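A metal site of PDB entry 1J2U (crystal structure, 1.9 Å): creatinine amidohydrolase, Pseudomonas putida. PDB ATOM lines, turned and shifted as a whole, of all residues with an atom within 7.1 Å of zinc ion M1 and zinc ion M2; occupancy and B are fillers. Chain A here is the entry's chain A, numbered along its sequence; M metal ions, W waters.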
ATOM      1  N   GLY A  31       2.016  29.802  26.627  1.00  0.00           N
ATOM      2  CA  GLY A  31       2.178  28.379  26.781  1.00  0.00           C
ATOM      3  C   GLY A  31       0.948  27.562  27.127  1.00  0.00           C
ATOM      4  O   GLY A  31      -0.135  27.780  26.602  1.00  0.00           O
ATOM      5  N   ALA A  32       1.152  26.569  27.983  1.00  0.00           N
ATOM      6  CA  ALA A  32       0.115  25.630  28.390  1.00  0.00           C
ATOM      7  C   ALA A  32       0.637  24.750  29.495  1.00  0.00           C
ATOM      8  O   ALA A  32       1.851  24.659  29.743  1.00  0.00           O
ATOM      9  CB  ALA A  32      -0.309  24.738  27.197  1.00  0.00           C
ATOM     10  N   LEU A  33      -0.307  24.116  30.190  1.00  0.00           N
ATOM     11  CA  LEU A  33      -0.026  23.084  31.170  1.00  0.00           C
ATOM     12  C   LEU A  33      -0.643  21.836  30.525  1.00  0.00           C
ATOM     13  O   LEU A  33      -1.875  21.718  30.405  1.00  0.00           O
ATOM     14  CB  LEU A  33      -0.646  23.396  32.537  1.00  0.00           C
ATOM     15  CG  LEU A  33      -0.397  22.315  33.609  1.00  0.00           C
ATOM     16  CD1 LEU A  33       1.085  22.209  33.969  1.00  0.00           C
ATOM     17  CD2 LEU A  33      -1.241  22.554  34.891  1.00  0.00           C
ATOM     18  N   GLU A  34       0.221  20.925  30.055  1.00  0.00           N
ATOM     19  CA  GLU A  34      -0.198  19.833  29.201  1.00  0.00           C
ATOM     20  C   GLU A  34       0.703  18.617  29.393  1.00  0.00           C
ATOM     21  O   GLU A  34       1.905  18.738  29.510  1.00  0.00           O
ATOM     22  CB  GLU A  34      -0.186  20.284  27.732  1.00  0.00           C
ATOM     23  CG  GLU A  34      -0.536  19.220  26.679  1.00  0.00           C
ATOM     24  CD  GLU A  34      -0.393  19.726  25.237  1.00  0.00           C
ATOM     25  OE1 GLU A  34      -1.297  19.528  24.389  1.00  0.00           O
ATOM     26  OE2 GLU A  34       0.645  20.337  24.959  1.00  0.00           O
ATOM     27  N   GLN A  35       0.099  17.449  29.447  1.00  0.00           N
ATOM     28  CA  GLN A  35       0.847  16.210  29.547  1.00  0.00           C
ATOM     29  C   GLN A  35       1.890  16.186  28.445  1.00  0.00           C
ATOM     30  O   GLN A  35       1.614  16.598  27.324  1.00  0.00           O
ATOM     31  CB  GLN A  35      -0.079  15.023  29.371  1.00  0.00           C
ATOM     32  CG  GLN A  35      -0.739  14.880  27.998  1.00  0.00           C
ATOM     33  CD  GLN A  35       0.100  14.080  27.010  1.00  0.00           C
ATOM     34  OE1 GLN A  35       1.043  13.405  27.406  1.00  0.00           O
ATOM     35  NE2 GLN A  35      -0.264  14.149  25.717  1.00  0.00           N
ATOM     36  N   HIS A  36       3.081  15.705  28.766  1.00  0.00           N
ATOM     37  CA  HIS A  36       4.139  15.520  27.788  1.00  0.00           C
ATOM     38  C   HIS A  36       4.778  14.130  27.969  1.00  0.00           C
ATOM     39  O   HIS A  36       5.990  14.031  28.102  1.00  0.00           O
ATOM     40  CB  HIS A  36       5.188  16.593  27.901  1.00  0.00           C
ATOM     41  CG  HIS A  36       4.849  17.851  27.169  1.00  0.00           C
ATOM     42  ND1 HIS A  36       3.915  18.755  27.627  1.00  0.00           N
ATOM     43  CD2 HIS A  36       5.314  18.358  26.002  1.00  0.00           C
ATOM     44  CE1 HIS A  36       3.813  19.758  26.773  1.00  0.00           C
ATOM     45  NE2 HIS A  36       4.655  19.534  25.773  1.00  0.00           N
ATOM     46  N   MET A  40       8.733  13.542  30.731  1.00  0.00           N
ATOM     47  CA  MET A  40       8.918  14.985  30.826  1.00  0.00           C
ATOM     48  C   MET A  40       7.782  15.602  31.612  1.00  0.00           C
ATOM     49  O   MET A  40       6.686  15.066  31.643  1.00  0.00           O
ATOM     50  CB  MET A  40       8.894  15.573  29.409  1.00  0.00           C
ATOM     51  CG  MET A  40       9.734  16.784  29.223  1.00  0.00           C
ATOM     52  SD  MET A  40      10.293  16.985  27.540  1.00  0.00           S
ATOM     53  CE  MET A  40       8.878  16.521  26.598  1.00  0.00           C
ATOM     54  N   MET A  42       4.972  18.758  32.795  1.00  0.00           N
ATOM     55  CA  MET A  42       3.829  19.351  32.092  1.00  0.00           C
ATOM     56  C   MET A  42       3.874  20.845  31.746  1.00  0.00           C
ATOM     57  O   MET A  42       3.010  21.331  31.003  1.00  0.00           O
ATOM     58  CB  MET A  42       2.538  19.014  32.861  1.00  0.00           C
ATOM     59  CG  MET A  42       2.251  17.510  32.882  1.00  0.00           C
ATOM     60  SD  MET A  42       0.641  17.122  33.603  1.00  0.00           S
ATOM     61  CE  MET A  42       0.949  17.448  35.287  1.00  0.00           C
ATOM     62  N   VAL A  44       6.354  22.305  30.047  1.00  0.00           N
ATOM     63  CA  VAL A  44       7.273  22.493  28.912  1.00  0.00           C
ATOM     64  C   VAL A  44       6.922  23.650  27.981  1.00  0.00           C
ATOM     65  O   VAL A  44       7.793  24.397  27.550  1.00  0.00           O
ATOM     66  CB  VAL A  44       7.361  21.163  28.102  1.00  0.00           C
ATOM     67  CG1 VAL A  44       7.977  21.353  26.727  1.00  0.00           C
ATOM     68  CG2 VAL A  44       8.117  20.111  28.912  1.00  0.00           C
ATOM     69  N   ASP A  45       5.649  23.792  27.648  1.00  0.00           N
ATOM     70  CA  ASP A  45       5.193  24.795  26.680  1.00  0.00           C
ATOM     71  C   ASP A  45       5.278  26.215  27.199  1.00  0.00           C
ATOM     72  O   ASP A  45       5.186  27.152  26.401  1.00  0.00           O
ATOM     73  CB  ASP A  45       3.795  24.486  26.183  1.00  0.00           C
ATOM     74  CG  ASP A  45       3.737  23.213  25.366  1.00  0.00           C
ATOM     75  OD1 ASP A  45       4.785  22.583  25.074  1.00  0.00           O
ATOM     76  OD2 ASP A  45       2.647  22.778  24.982  1.00  0.00           O
ATOM     77  N   VAL A  46       5.431  26.363  28.513  1.00  0.00           N
ATOM     78  CA  VAL A  46       5.771  27.664  29.110  1.00  0.00           C
ATOM     79  C   VAL A  46       7.302  27.820  29.190  1.00  0.00           C
ATOM     80  O   VAL A  46       7.859  28.841  28.778  1.00  0.00           O
ATOM     81  CB  VAL A  46       5.205  27.843  30.539  1.00  0.00           C
ATOM     82  CG1 VAL A  46       5.671  29.174  31.110  1.00  0.00           C
ATOM     83  CG2 VAL A  46       3.688  27.735  30.546  1.00  0.00           C
ATOM     84  N   LEU A  48       9.892  26.461  27.597  1.00  0.00           N
ATOM     85  CA  LEU A  48      10.645  26.571  26.358  1.00  0.00           C
ATOM     86  C   LEU A  48      10.551  27.951  25.665  1.00  0.00           C
ATOM     87  O   LEU A  48      11.573  28.595  25.456  1.00  0.00           O
ATOM     88  CB  LEU A  48      10.272  25.405  25.443  1.00  0.00           C
ATOM     89  CG  LEU A  48      10.718  24.052  26.002  1.00  0.00           C
ATOM     90  CD1 LEU A  48      10.569  22.965  24.972  1.00  0.00           C
ATOM     91  CD2 LEU A  48      12.152  24.036  26.540  1.00  0.00           C
ATOM     92  N   TYR A  72      -5.024  26.790  25.153  1.00  0.00           N
ATOM     93  CA  TYR A  72      -6.187  26.183  24.553  1.00  0.00           C
ATOM     94  C   TYR A  72      -6.157  24.648  24.709  1.00  0.00           C
ATOM     95  O   TYR A  72      -5.065  24.043  24.842  1.00  0.00           O
ATOM     96  CB  TYR A  72      -6.423  26.607  23.088  1.00  0.00           C
ATOM     97  CG  TYR A  72      -7.740  26.092  22.607  1.00  0.00           C
ATOM     98  CD1 TYR A  72      -8.927  26.536  23.173  1.00  0.00           C
ATOM     99  CD2 TYR A  72      -7.819  25.092  21.641  1.00  0.00           C
ATOM    100  CE1 TYR A  72     -10.145  26.031  22.771  1.00  0.00           C
ATOM    101  CE2 TYR A  72      -9.020  24.566  21.247  1.00  0.00           C
ATOM    102  CZ  TYR A  72     -10.189  25.027  21.815  1.00  0.00           C
ATOM    103  OH  TYR A  72     -11.384  24.484  21.414  1.00  0.00           O
ATOM    104  N   SER A  74      -5.892  20.855  24.448  1.00  0.00           N
ATOM    105  CA  SER A  74      -5.055  19.932  23.693  1.00  0.00           C
ATOM    106  C   SER A  74      -5.893  19.150  22.666  1.00  0.00           C
ATOM    107  O   SER A  74      -6.974  18.619  23.015  1.00  0.00           O
ATOM    108  CB  SER A  74      -4.397  18.966  24.680  1.00  0.00           C
ATOM    109  OG  SER A  74      -3.629  17.976  24.027  1.00  0.00           O
ATOM    110  N   SER A  78      -2.326  16.839  17.682  1.00  0.00           N
ATOM    111  CA  SER A  78      -1.197  17.718  17.965  1.00  0.00           C
ATOM    112  C   SER A  78      -0.679  17.721  19.421  1.00  0.00           C
ATOM    113  O   SER A  78       0.404  18.255  19.702  1.00  0.00           O
ATOM    114  CB  SER A  78      -1.545  19.156  17.575  1.00  0.00           C
ATOM    115  OG  SER A  78      -2.765  19.575  18.149  1.00  0.00           O
ATOM    116  N   GLY A  79      -1.444  17.118  20.341  1.00  0.00           N
ATOM    117  CA  GLY A  79      -1.080  17.089  21.755  1.00  0.00           C
ATOM    118  C   GLY A  79      -1.632  15.916  22.551  1.00  0.00           C
ATOM    119  O   GLY A  79      -1.584  15.928  23.781  1.00  0.00           O
ATOM    120  N   GLY A 119       4.185  28.676  22.412  1.00  0.00           N
ATOM    121  CA  GLY A 119       4.866  27.431  22.713  1.00  0.00           C
ATOM    122  C   GLY A 119       3.990  26.205  22.746  1.00  0.00           C
ATOM    123  O   GLY A 119       4.498  25.104  22.976  1.00  0.00           O
ATOM    124  N   HIS A 120       2.697  26.387  22.461  1.00  0.00           N
ATOM    125  CA  HIS A 120       1.677  25.310  22.514  1.00  0.00           C
ATOM    126  C   HIS A 120       0.912  25.351  21.214  1.00  0.00           C
ATOM    127  O   HIS A 120       0.288  26.363  20.865  1.00  0.00           O
ATOM    128  CB  HIS A 120       0.783  25.570  23.737  1.00  0.00           C
ATOM    129  CG  HIS A 120      -0.405  24.668  23.860  1.00  0.00           C
ATOM    130  ND1 HIS A 120      -0.309  23.300  24.047  1.00  0.00           N
ATOM    131  CD2 HIS A 120      -1.727  24.960  23.905  1.00  0.00           C
ATOM    132  CE1 HIS A 120      -1.526  22.791  24.186  1.00  0.00           C
ATOM    133  NE2 HIS A 120      -2.407  23.785  24.104  1.00  0.00           N
ATOM    134  N   TYR A 121       0.994  24.261  20.477  1.00  0.00           N
ATOM    135  CA  TYR A 121       0.508  24.200  19.100  1.00  0.00           C
ATOM    136  C   TYR A 121      -0.913  24.710  18.906  1.00  0.00           C
ATOM    137  O   TYR A 121      -1.176  25.486  17.980  1.00  0.00           O
ATOM    138  CB  TYR A 121       0.608  22.763  18.603  1.00  0.00           C
ATOM    139  CG  TYR A 121       0.475  22.603  17.121  1.00  0.00           C
ATOM    140  CD1 TYR A 121       1.596  22.597  16.305  1.00  0.00           C
ATOM    141  CD2 TYR A 121      -0.771  22.482  16.519  1.00  0.00           C
ATOM    142  CE1 TYR A 121       1.491  22.451  14.943  1.00  0.00           C
ATOM    143  CE2 TYR A 121      -0.895  22.351  15.161  1.00  0.00           C
ATOM    144  CZ  TYR A 121       0.255  22.321  14.369  1.00  0.00           C
ATOM    145  OH  TYR A 121       0.189  22.184  12.992  1.00  0.00           O
ATOM    146  N   GLU A 122      -1.806  24.339  19.825  1.00  0.00           N
ATOM    147  CA  GLU A 122      -3.213  24.681  19.742  1.00  0.00           C
ATOM    148  C   GLU A 122      -3.622  26.128  20.056  1.00  0.00           C
ATOM    149  O   GLU A 122      -4.776  26.502  19.776  1.00  0.00           O
ATOM    150  CB  GLU A 122      -3.984  23.739  20.707  1.00  0.00           C
ATOM    151  CG  GLU A 122      -3.987  22.281  20.258  1.00  0.00           C
ATOM    152  CD  GLU A 122      -2.829  21.452  20.781  1.00  0.00           C
ATOM    153  OE1 GLU A 122      -1.836  22.020  21.287  1.00  0.00           O
ATOM    154  OE2 GLU A 122      -2.928  20.205  20.695  1.00  0.00           O
ATOM    155  N   TYR A 153       7.824  29.273  18.022  1.00  0.00           N
ATOM    156  CA  TYR A 153       9.297  29.279  17.954  1.00  0.00           C
ATOM    157  C   TYR A 153       9.883  28.157  17.099  1.00  0.00           C
ATOM    158  O   TYR A 153      10.910  28.374  16.431  1.00  0.00           O
ATOM    159  CB  TYR A 153       9.941  29.354  19.341  1.00  0.00           C
ATOM    160  CG  TYR A 153       9.822  28.091  20.126  1.00  0.00           C
ATOM    161  CD1 TYR A 153      10.807  27.128  20.085  1.00  0.00           C
ATOM    162  CD2 TYR A 153       8.690  27.842  20.892  1.00  0.00           C
ATOM    163  CE1 TYR A 153      10.692  25.939  20.779  1.00  0.00           C
ATOM    164  CE2 TYR A 153       8.557  26.654  21.599  1.00  0.00           C
ATOM    165  CZ  TYR A 153       9.553  25.707  21.528  1.00  0.00           C
ATOM    166  OH  TYR A 153       9.443  24.532  22.221  1.00  0.00           O
ATOM    167  N   TRP A 154       9.246  26.989  17.102  1.00  0.00           N
ATOM    168  CA  TRP A 154       9.724  25.869  16.290  1.00  0.00           C
ATOM    169  C   TRP A 154       9.700  26.097  14.783  1.00  0.00           C
ATOM    170  O   TRP A 154      10.489  25.477  14.054  1.00  0.00           O
ATOM    171  CB  TRP A 154       8.937  24.603  16.590  1.00  0.00           C
ATOM    172  CG  TRP A 154       7.461  24.738  16.433  1.00  0.00           C
ATOM    173  CD1 TRP A 154       6.723  24.647  15.278  1.00  0.00           C
ATOM    174  CD2 TRP A 154       6.517  24.964  17.484  1.00  0.00           C
ATOM    175  NE1 TRP A 154       5.382  24.785  15.563  1.00  0.00           N
ATOM    176  CE2 TRP A 154       5.226  25.010  16.907  1.00  0.00           C
ATOM    177  CE3 TRP A 154       6.627  25.139  18.860  1.00  0.00           C
ATOM    178  CZ2 TRP A 154       4.067  25.212  17.661  1.00  0.00           C
ATOM    179  CZ3 TRP A 154       5.479  25.359  19.609  1.00  0.00           C
ATOM    180  CH2 TRP A 154       4.222  25.384  19.002  1.00  0.00           C
ATOM    181  N   GLU A 177       4.976  16.348  16.437  1.00  0.00           N
ATOM    182  CA  GLU A 177       6.036  16.635  17.385  1.00  0.00           C
ATOM    183  C   GLU A 177       5.381  17.118  18.671  1.00  0.00           C
ATOM    184  O   GLU A 177       5.213  18.339  18.877  1.00  0.00           O
ATOM    185  CB  GLU A 177       6.966  17.765  16.929  1.00  0.00           C
ATOM    186  CG  GLU A 177       8.262  17.345  16.285  1.00  0.00           C
ATOM    187  CD  GLU A 177       9.014  16.301  17.074  1.00  0.00           C
ATOM    188  OE1 GLU A 177       9.193  15.222  16.519  1.00  0.00           O
ATOM    189  OE2 GLU A 177       9.414  16.561  18.236  1.00  0.00           O
ATOM    190  N   HIS A 178       4.954  16.182  19.491  1.00  0.00           N
ATOM    191  CA  HIS A 178       4.508  16.521  20.822  1.00  0.00           C
ATOM    192  C   HIS A 178       5.215  15.547  21.733  1.00  0.00           C
ATOM    193  O   HIS A 178       4.985  14.346  21.652  1.00  0.00           O
ATOM    194  CB  HIS A 178       3.005  16.383  20.989  1.00  0.00           C
ATOM    195  CG  HIS A 178       2.559  16.504  22.406  1.00  0.00           C
ATOM    196  ND1 HIS A 178       2.671  17.677  23.127  1.00  0.00           N
ATOM    197  CD2 HIS A 178       2.004  15.598  23.241  1.00  0.00           C
ATOM    198  CE1 HIS A 178       2.217  17.479  24.353  1.00  0.00           C
ATOM    199  NE2 HIS A 178       1.801  16.234  24.441  1.00  0.00           N
ATOM    200  N   GLY A 179       6.087  16.078  22.576  1.00  0.00           N
ATOM    201  CA  GLY A 179       6.838  15.295  23.526  1.00  0.00           C
ATOM    202  C   GLY A 179       7.925  14.445  22.899  1.00  0.00           C
ATOM    203  O   GLY A 179       8.424  13.515  23.546  1.00  0.00           O
ATOM    204  N   GLU A 183      11.221  18.822  21.529  1.00  0.00           N
ATOM    205  CA  GLU A 183      11.051  19.374  22.867  1.00  0.00           C
ATOM    206  C   GLU A 183      11.947  18.720  23.896  1.00  0.00           C
ATOM    207  O   GLU A 183      12.474  19.380  24.781  1.00  0.00           O
ATOM    208  CB  GLU A 183       9.586  19.245  23.311  1.00  0.00           C
ATOM    209  CG  GLU A 183       8.662  20.140  22.549  1.00  0.00           C
ATOM    210  CD  GLU A 183       7.238  20.063  23.085  1.00  0.00           C
ATOM    211  OE1 GLU A 183       6.706  21.119  23.421  1.00  0.00           O
ATOM    212  OE2 GLU A 183       6.677  18.949  23.154  1.00  0.00           O
HETATM  213 ZN    ZN M   1       4.863  20.809  24.204  1.00  0.00          ZN
HETATM  214 ZN    ZN M   2       1.386  21.750  23.748  1.00  0.00          ZN
HETATM  215  O   HOH W   1       1.801  21.930  22.029  1.00  0.00           O
HETATM  216  O   HOH W   2       0.171  20.283  21.984  1.00  0.00           O
HETATM  217  O   HOH W   3       3.684  20.411  22.946  1.00  0.00           O
HETATM  218  O   HOH W   4       4.433  22.612  21.681  1.00  0.00           O
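ND1 of His 178 touches zinc ion M1, 3.97 Å away.
Of the 26 residues printed, 4 come within 4 Å of zinc ion M1.
Within 4 Å of zinc ion M2: Glu 34, Asp 45 and His 120.
Zinc ion M1 is bound by water W3 (1.8 Å), the side-chain carboxylate (OD1) of Asp 45 (2.0 Å), the side-chain carboxylate (OE1) of Glu 183 (2.0 Å) and a ring nitrogen (NE2) of His 36 (2.0 Å).
Zinc ion M1 has four donor atoms within binding distance.
Slightly farther from zinc ion M1 lies the side-chain carboxylate (OE2) of Glu 183 (2.8 Å).
Water W3 bridges a ring nitrogen (ND1) of His 178 (2.9 Å) and the side-chain carboxylate (OE2) of Glu 183 (3.3 Å).
Zinc ion M2 is bound by water W1 (1.8 Å), the side-chain carboxylate of Glu 34 (2.0 Å), the side-chain carboxylate of Asp 45 (2.0 Å), a ring nitrogen (ND1) of His 120 (2.3 Å) and water W2 (2.6 Å).
Slightly farther from zinc ion M2 lies water W3 (2.8 Å).
The backbone carbonyl oxygen of Glu 34 lies within hydrogen-bond range of a ring nitrogen (ND1) of His 36, 2.8 Å away.
The side-chain hydroxyl of Ser 74 lies within hydrogen-bond range of the side-chain carboxylate of Glu 34 (2.8 Å).
The backbone NH of Glu 34 lies within hydrogen-bond range of the backbone carbonyl oxygen of Met 42 (3.0 Å).
OE2 of Glu 183 lies within hydrogen-bond range of N of Gly 179, 3.0 Å away.
OE1 of Glu 122 sits close to NE2 of His 120.
NE2 of His 120 lies within hydrogen-bond range of O of Tyr 72 (2.8 Å).
A ring nitrogen (NE2) of His 178 is in hydrogen-bond range of the backbone carbonyl oxygen of Gly 79.
A ring nitrogen (NE2) of His 178 sits at hydrogen-bond distance from the backbone carbonyl oxygen (O) of Gln 35, 2.9 Å away.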
